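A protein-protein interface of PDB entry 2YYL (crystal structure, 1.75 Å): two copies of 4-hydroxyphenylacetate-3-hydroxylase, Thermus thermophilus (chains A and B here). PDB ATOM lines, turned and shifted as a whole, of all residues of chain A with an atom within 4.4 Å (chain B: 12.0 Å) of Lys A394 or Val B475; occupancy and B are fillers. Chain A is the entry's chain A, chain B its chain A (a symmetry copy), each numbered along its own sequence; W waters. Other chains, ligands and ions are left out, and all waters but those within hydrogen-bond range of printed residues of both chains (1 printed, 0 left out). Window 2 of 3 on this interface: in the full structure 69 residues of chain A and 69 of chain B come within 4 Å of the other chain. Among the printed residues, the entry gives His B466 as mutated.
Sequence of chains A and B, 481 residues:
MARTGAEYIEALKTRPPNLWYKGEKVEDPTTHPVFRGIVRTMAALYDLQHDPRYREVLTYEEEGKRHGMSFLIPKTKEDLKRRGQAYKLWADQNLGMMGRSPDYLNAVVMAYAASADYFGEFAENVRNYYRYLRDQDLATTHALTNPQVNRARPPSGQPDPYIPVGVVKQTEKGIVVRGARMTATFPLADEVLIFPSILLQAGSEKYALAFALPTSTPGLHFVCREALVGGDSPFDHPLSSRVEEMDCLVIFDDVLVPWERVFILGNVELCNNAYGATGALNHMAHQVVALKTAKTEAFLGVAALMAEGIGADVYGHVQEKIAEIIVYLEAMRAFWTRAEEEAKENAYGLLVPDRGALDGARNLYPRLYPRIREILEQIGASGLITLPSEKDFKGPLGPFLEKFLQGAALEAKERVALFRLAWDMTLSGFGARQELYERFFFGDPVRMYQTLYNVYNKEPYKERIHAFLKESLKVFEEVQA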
ATOM      1  N   PRO A 234      -0.480 -17.584  -3.619  1.00  0.00           N
ATOM      2  CA  PRO A 234      -0.101 -18.780  -2.862  1.00  0.00           C
ATOM      3  C   PRO A 234      -0.144 -18.507  -1.354  1.00  0.00           C
ATOM      4  O   PRO A 234      -0.354 -19.420  -0.557  1.00  0.00           O
ATOM      5  CB  PRO A 234       1.308 -19.081  -3.372  1.00  0.00           C
ATOM      6  CG  PRO A 234       1.824 -17.720  -3.776  1.00  0.00           C
ATOM      7  CD  PRO A 234       0.631 -17.125  -4.473  1.00  0.00           C
ATOM      8  N   PHE A 235       0.054 -17.250  -0.964  1.00  0.00           N
ATOM      9  CA  PHE A 235       0.015 -16.884   0.452  1.00  0.00           C
ATOM     10  C   PHE A 235      -1.427 -16.950   0.949  1.00  0.00           C
ATOM     11  O   PHE A 235      -1.717 -17.587   1.957  1.00  0.00           O
ATOM     12  CB  PHE A 235       0.552 -15.461   0.660  1.00  0.00           C
ATOM     13  CG  PHE A 235       0.577 -15.018   2.104  1.00  0.00           C
ATOM     14  CD1 PHE A 235       1.695 -15.251   2.900  1.00  0.00           C
ATOM     15  CD2 PHE A 235      -0.520 -14.377   2.665  1.00  0.00           C
ATOM     16  CE1 PHE A 235       1.723 -14.849   4.238  1.00  0.00           C
ATOM     17  CE2 PHE A 235      -0.506 -13.967   4.006  1.00  0.00           C
ATOM     18  CZ  PHE A 235       0.621 -14.207   4.792  1.00  0.00           C
ATOM     19  N   GLU A 390      -1.995 -11.095   2.109  1.00  0.00           N
ATOM     20  CA  GLU A 390      -0.632 -10.644   1.883  1.00  0.00           C
ATOM     21  C   GLU A 390      -0.751  -9.151   1.564  1.00  0.00           C
ATOM     22  O   GLU A 390       0.170  -8.374   1.811  1.00  0.00           O
ATOM     23  CB  GLU A 390      -0.001 -11.379   0.695  1.00  0.00           C
ATOM     24  CG  GLU A 390      -0.886 -11.457  -0.539  1.00  0.00           C
ATOM     25  CD  GLU A 390      -0.079 -11.536  -1.819  1.00  0.00           C
ATOM     26  OE1 GLU A 390       0.641 -10.561  -2.115  1.00  0.00           O
ATOM     27  OE2 GLU A 390      -0.158 -12.563  -2.529  1.00  0.00           O
ATOM     28  N   LYS A 391      -1.904  -8.760   1.026  1.00  0.00           N
ATOM     29  CA  LYS A 391      -2.149  -7.363   0.676  1.00  0.00           C
ATOM     30  C   LYS A 391      -2.200  -6.477   1.916  1.00  0.00           C
ATOM     31  O   LYS A 391      -1.838  -5.298   1.866  1.00  0.00           O
ATOM     32  CB  LYS A 391      -3.449  -7.233  -0.124  1.00  0.00           C
ATOM     33  CG  LYS A 391      -3.356  -7.832  -1.519  1.00  0.00           C
ATOM     34  CD  LYS A 391      -4.607  -7.563  -2.335  1.00  0.00           C
ATOM     35  CE  LYS A 391      -4.443  -8.066  -3.760  1.00  0.00           C
ATOM     36  NZ  LYS A 391      -5.660  -7.812  -4.582  1.00  0.00           N
ATOM     37  N   ASP A 392      -2.651  -7.040   3.034  1.00  0.00           N
ATOM     38  CA  ASP A 392      -2.710  -6.277   4.276  1.00  0.00           C
ATOM     39  C   ASP A 392      -1.295  -6.068   4.803  1.00  0.00           C
ATOM     40  O   ASP A 392      -0.969  -5.000   5.325  1.00  0.00           O
ATOM     41  CB  ASP A 392      -3.561  -7.009   5.316  1.00  0.00           C
ATOM     42  CG  ASP A 392      -5.032  -6.990   4.973  1.00  0.00           C
ATOM     43  OD1 ASP A 392      -5.628  -5.891   4.972  1.00  0.00           O
ATOM     44  OD2 ASP A 392      -5.594  -8.071   4.694  1.00  0.00           O
ATOM     45  N   PHE A 393      -0.453  -7.088   4.660  1.00  0.00           N
ATOM     46  CA  PHE A 393       0.930  -6.996   5.112  1.00  0.00           C
ATOM     47  C   PHE A 393       1.706  -6.002   4.258  1.00  0.00           C
ATOM     48  O   PHE A 393       2.632  -5.347   4.739  1.00  0.00           O
ATOM     49  CB  PHE A 393       1.609  -8.365   5.047  1.00  0.00           C
ATOM     50  CG  PHE A 393       1.391  -9.204   6.272  1.00  0.00           C
ATOM     51  CD1 PHE A 393       1.983  -8.854   7.480  1.00  0.00           C
ATOM     52  CD2 PHE A 393       0.580 -10.330   6.225  1.00  0.00           C
ATOM     53  CE1 PHE A 393       1.775  -9.617   8.626  1.00  0.00           C
ATOM     54  CE2 PHE A 393       0.366 -11.099   7.364  1.00  0.00           C
ATOM     55  CZ  PHE A 393       0.961 -10.742   8.566  1.00  0.00           C
ATOM     56  N   LYS A 394       1.317  -5.897   2.992  1.00  0.00           N
ATOM     57  CA  LYS A 394       1.970  -4.988   2.054  1.00  0.00           C
ATOM     58  C   LYS A 394       1.361  -3.590   2.118  1.00  0.00           C
ATOM     59  O   LYS A 394       1.868  -2.654   1.494  1.00  0.00           O
ATOM     60  CB  LYS A 394       1.851  -5.526   0.625  1.00  0.00           C
ATOM     61  CG  LYS A 394       2.598  -6.822   0.381  1.00  0.00           C
ATOM     62  CD  LYS A 394       2.370  -7.333  -1.032  1.00  0.00           C
ATOM     63  CE  LYS A 394       3.146  -8.616  -1.287  1.00  0.00           C
ATOM     64  NZ  LYS A 394       2.892  -9.154  -2.650  1.00  0.00           N
ATOM     65  N   GLY A 395       0.274  -3.459   2.871  1.00  0.00           N
ATOM     66  CA  GLY A 395      -0.397  -2.179   2.997  1.00  0.00           C
ATOM     67  C   GLY A 395       0.066  -1.345   4.179  1.00  0.00           C
ATOM     68  O   GLY A 395       0.993  -1.727   4.893  1.00  0.00           O
ATOM     69  N   HIS B 466       7.156 -26.499   6.046  1.00  0.00           N
ATOM     70  CA  HIS B 466       7.956 -25.290   5.882  1.00  0.00           C
ATOM     71  C   HIS B 466       8.364 -25.158   4.419  1.00  0.00           C
ATOM     72  O   HIS B 466       8.342 -24.063   3.856  1.00  0.00           O
ATOM     73  CB  HIS B 466       9.183 -25.337   6.802  1.00  0.00           C
ATOM     74  CG  HIS B 466       8.898 -24.881   8.199  1.00  0.00           C
ATOM     75  ND1 HIS B 466       9.602 -25.336   9.294  1.00  0.00           N
ATOM     76  CD2 HIS B 466       7.993 -23.993   8.678  1.00  0.00           C
ATOM     77  CE1 HIS B 466       9.143 -24.750  10.386  1.00  0.00           C
ATOM     78  NE2 HIS B 466       8.167 -23.930  10.040  1.00  0.00           N
ATOM     79  N   ALA B 467       8.709 -26.280   3.797  1.00  0.00           N
ATOM     80  CA  ALA B 467       9.096 -26.272   2.391  1.00  0.00           C
ATOM     81  C   ALA B 467       7.907 -25.852   1.533  1.00  0.00           C
ATOM     82  O   ALA B 467       8.050 -25.070   0.597  1.00  0.00           O
ATOM     83  CB  ALA B 467       9.576 -27.657   1.970  1.00  0.00           C
ATOM     84  N   PHE B 468       6.726 -26.367   1.860  1.00  0.00           N
ATOM     85  CA  PHE B 468       5.531 -26.034   1.094  1.00  0.00           C
ATOM     86  C   PHE B 468       5.176 -24.559   1.222  1.00  0.00           C
ATOM     87  O   PHE B 468       4.685 -23.947   0.274  1.00  0.00           O
ATOM     88  CB  PHE B 468       4.337 -26.876   1.561  1.00  0.00           C
ATOM     89  CG  PHE B 468       3.190 -26.880   0.589  1.00  0.00           C
ATOM     90  CD1 PHE B 468       3.158 -27.794  -0.460  1.00  0.00           C
ATOM     91  CD2 PHE B 468       2.164 -25.942   0.692  1.00  0.00           C
ATOM     92  CE1 PHE B 468       2.123 -27.778  -1.394  1.00  0.00           C
ATOM     93  CE2 PHE B 468       1.122 -25.915  -0.237  1.00  0.00           C
ATOM     94  CZ  PHE B 468       1.104 -26.834  -1.284  1.00  0.00           C
ATOM     95  N   LEU B 469       5.427 -23.985   2.395  1.00  0.00           N
ATOM     96  CA  LEU B 469       5.107 -22.588   2.641  1.00  0.00           C
ATOM     97  C   LEU B 469       6.092 -21.595   2.025  1.00  0.00           C
ATOM     98  O   LEU B 469       5.847 -20.392   2.043  1.00  0.00           O
ATOM     99  CB  LEU B 469       4.990 -22.334   4.149  1.00  0.00           C
ATOM    100  CG  LEU B 469       3.791 -23.009   4.834  1.00  0.00           C
ATOM    101  CD1 LEU B 469       3.836 -22.763   6.342  1.00  0.00           C
ATOM    102  CD2 LEU B 469       2.498 -22.465   4.238  1.00  0.00           C
ATOM    103  N   LYS B 470       7.201 -22.088   1.481  1.00  0.00           N
ATOM    104  CA  LYS B 470       8.175 -21.187   0.866  1.00  0.00           C
ATOM    105  C   LYS B 470       7.517 -20.353  -0.229  1.00  0.00           C
ATOM    106  O   LYS B 470       7.787 -19.156  -0.357  1.00  0.00           O
ATOM    107  CB  LYS B 470       9.348 -21.976   0.278  1.00  0.00           C
ATOM    108  CG  LYS B 470      10.320 -22.512   1.313  1.00  0.00           C
ATOM    109  CD  LYS B 470      11.543 -23.114   0.635  1.00  0.00           C
ATOM    110  CE  LYS B 470      12.600 -23.528   1.643  1.00  0.00           C
ATOM    111  NZ  LYS B 470      13.791 -24.120   0.969  1.00  0.00           N
ATOM    112  N   GLU B 471       6.647 -20.986  -1.009  1.00  0.00           N
ATOM    113  CA  GLU B 471       5.951 -20.301  -2.095  1.00  0.00           C
ATOM    114  C   GLU B 471       5.042 -19.199  -1.549  1.00  0.00           C
ATOM    115  O   GLU B 471       4.821 -18.178  -2.207  1.00  0.00           O
ATOM    116  CB  GLU B 471       5.120 -21.303  -2.896  1.00  0.00           C
ATOM    117  CG  GLU B 471       4.714 -20.813  -4.273  1.00  0.00           C
ATOM    118  CD  GLU B 471       5.912 -20.563  -5.174  1.00  0.00           C
ATOM    119  OE1 GLU B 471       6.764 -21.469  -5.303  1.00  0.00           O
ATOM    120  OE2 GLU B 471       5.998 -19.463  -5.759  1.00  0.00           O
ATOM    121  N   SER B 472       4.511 -19.412  -0.350  1.00  0.00           N
ATOM    122  CA  SER B 472       3.638 -18.428   0.279  1.00  0.00           C
ATOM    123  C   SER B 472       4.414 -17.168   0.645  1.00  0.00           C
ATOM    124  O   SER B 472       3.983 -16.051   0.355  1.00  0.00           O
ATOM    125  CB  SER B 472       3.005 -19.005   1.549  1.00  0.00           C
ATOM    126  OG  SER B 472       2.148 -20.086   1.239  1.00  0.00           O
ATOM    127  N   LEU B 473       5.562 -17.357   1.289  1.00  0.00           N
ATOM    128  CA  LEU B 473       6.388 -16.234   1.722  1.00  0.00           C
ATOM    129  C   LEU B 473       7.091 -15.520   0.574  1.00  0.00           C
ATOM    130  O   LEU B 473       7.549 -14.389   0.732  1.00  0.00           O
ATOM    131  CB  LEU B 473       7.424 -16.704   2.748  1.00  0.00           C
ATOM    132  CG  LEU B 473       6.933 -17.080   4.157  1.00  0.00           C
ATOM    133  CD1 LEU B 473       6.284 -15.872   4.809  1.00  0.00           C
ATOM    134  CD2 LEU B 473       5.952 -18.231   4.087  1.00  0.00           C
ATOM    135  N   LYS B 474       7.166 -16.175  -0.578  1.00  0.00           N
ATOM    136  CA  LYS B 474       7.831 -15.592  -1.741  1.00  0.00           C
ATOM    137  C   LYS B 474       7.076 -14.400  -2.335  1.00  0.00           C
ATOM    138  O   LYS B 474       7.653 -13.612  -3.083  1.00  0.00           O
ATOM    139  CB  LYS B 474       8.037 -16.669  -2.810  1.00  0.00           C
ATOM    140  CG  LYS B 474       8.943 -16.254  -3.958  1.00  0.00           C
ATOM    141  CD  LYS B 474       9.195 -17.420  -4.905  1.00  0.00           C
ATOM    142  CE  LYS B 474      10.173 -17.038  -6.005  1.00  0.00           C
ATOM    143  NZ  LYS B 474      10.415 -18.162  -6.954  1.00  0.00           N
ATOM    144  N   VAL B 475       5.797 -14.258  -2.003  1.00  0.00           N
ATOM    145  CA  VAL B 475       5.008 -13.147  -2.532  1.00  0.00           C
ATOM    146  C   VAL B 475       5.494 -11.803  -2.001  1.00  0.00           C
ATOM    147  O   VAL B 475       5.122 -10.750  -2.523  1.00  0.00           O
ATOM    148  CB  VAL B 475       3.506 -13.284  -2.181  1.00  0.00           C
ATOM    149  CG1 VAL B 475       2.972 -14.625  -2.682  1.00  0.00           C
ATOM    150  CG2 VAL B 475       3.302 -13.134  -0.671  1.00  0.00           C
ATOM    151  N   PHE B 476       6.324 -11.837  -0.966  1.00  0.00           N
ATOM    152  CA  PHE B 476       6.840 -10.608  -0.374  1.00  0.00           C
ATOM    153  C   PHE B 476       8.202 -10.210  -0.927  1.00  0.00           C
ATOM    154  O   PHE B 476       8.723  -9.148  -0.590  1.00  0.00           O
ATOM    155  CB  PHE B 476       6.917 -10.755   1.145  1.00  0.00           C
ATOM    156  CG  PHE B 476       5.587 -11.015   1.790  1.00  0.00           C
ATOM    157  CD1 PHE B 476       4.583 -10.051   1.758  1.00  0.00           C
ATOM    158  CD2 PHE B 476       5.325 -12.235   2.405  1.00  0.00           C
ATOM    159  CE1 PHE B 476       3.336 -10.299   2.330  1.00  0.00           C
ATOM    160  CE2 PHE B 476       4.083 -12.492   2.978  1.00  0.00           C
ATOM    161  CZ  PHE B 476       3.086 -11.525   2.940  1.00  0.00           C
ATOM    162  N   GLU B 477       8.774 -11.062  -1.772  1.00  0.00           N
ATOM    163  CA  GLU B 477      10.076 -10.775  -2.367  1.00  0.00           C
ATOM    164  C   GLU B 477       9.949  -9.697  -3.435  1.00  0.00           C
ATOM    165  O   GLU B 477       8.808  -9.422  -3.868  1.00  0.00           O
ATOM    166  CB  GLU B 477      10.674 -12.039  -2.994  1.00  0.00           C
ATOM    167  CG  GLU B 477      11.105 -13.097  -1.993  1.00  0.00           C
ATOM    168  CD  GLU B 477      11.800 -14.277  -2.652  1.00  0.00           C
ATOM    169  OE1 GLU B 477      12.265 -15.180  -1.923  1.00  0.00           O
ATOM    170  OE2 GLU B 477      11.883 -14.304  -3.899  1.00  0.00           O
HETATM  171  O   HOH W   1       0.015 -19.574   2.902  1.00  0.00           O
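Among the printed residues, merely in contact across the chains: Pro A234 with Glu B471, Pro A234 with Val B475, Phe A235 with Ser B472, Phe A235 with Phe B476, Lys A394 with Phe B476, Glu A390 with Phe B476, Glu A390 with Val B475, Phe A393 with Phe B476 and Phe A235 with Val B475.
No position is printed for both chains. Of the 11 pairs that touch across the chains among the printed residues, none has its exchanged pair printed and touching as well.
Of chain B, only Val B475 and Phe B476 come within 4 Å of Lys A394. Glu A390 touches two residues of chain B. Asp A392 touches none of the printed residues of chain B. No residue of chain B comes within 4 Å of Gly A395. Of the printed residues of chain A, Ser B472 touches Pro A234 (3.2 Å) and Phe A235 (3.5 Å). Of the printed residues of chain A, Phe B476 touches Phe A235 (3.6 Å), Glu A390 (3.7 Å), Phe A393 (3.8 Å) and Lys A394 (3.7 Å). Printed residues of chain A within 4 Å of Glu B471: Pro A234. The nearest residue of chain B that does not touch Lys A394 is Glu B477 (6.0 Å).
The side-chain amino group (NZ) of Lys A394 lies within salt-bridge range of the side-chain carboxylate (OE1) of Glu A390.
O of Pro A234 lies within hydrogen-bond range of OG of Ser B472 (3.2 Å). The side-chain amino group (NZ) of Lys A394 sits at hydrogen-bond distance from the backbone carbonyl oxygen (O) of Val B475, at 2.7 Å.
Of the 8 printed residues of chain A, 5 touch a printed residue of chain B. Of the 12 printed residues of chain B, 4 touch a printed residue of chain A. Along chain B the printed residues that touch a printed residue of chain A span positions 471 to 476. Among the printed residues, 11 pairs touch across the chains. Among the printed residues, no Asp or Glu carboxylate lies within 4 Å of a Lys or Arg side-chain nitrogen of the other chain.
Water W1 lies within hydrogen-bond range of OG of Ser B472 (2.8 Å), O of Phe A235 (2.8 Å) and O of Pro A234 (3.5 Å).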
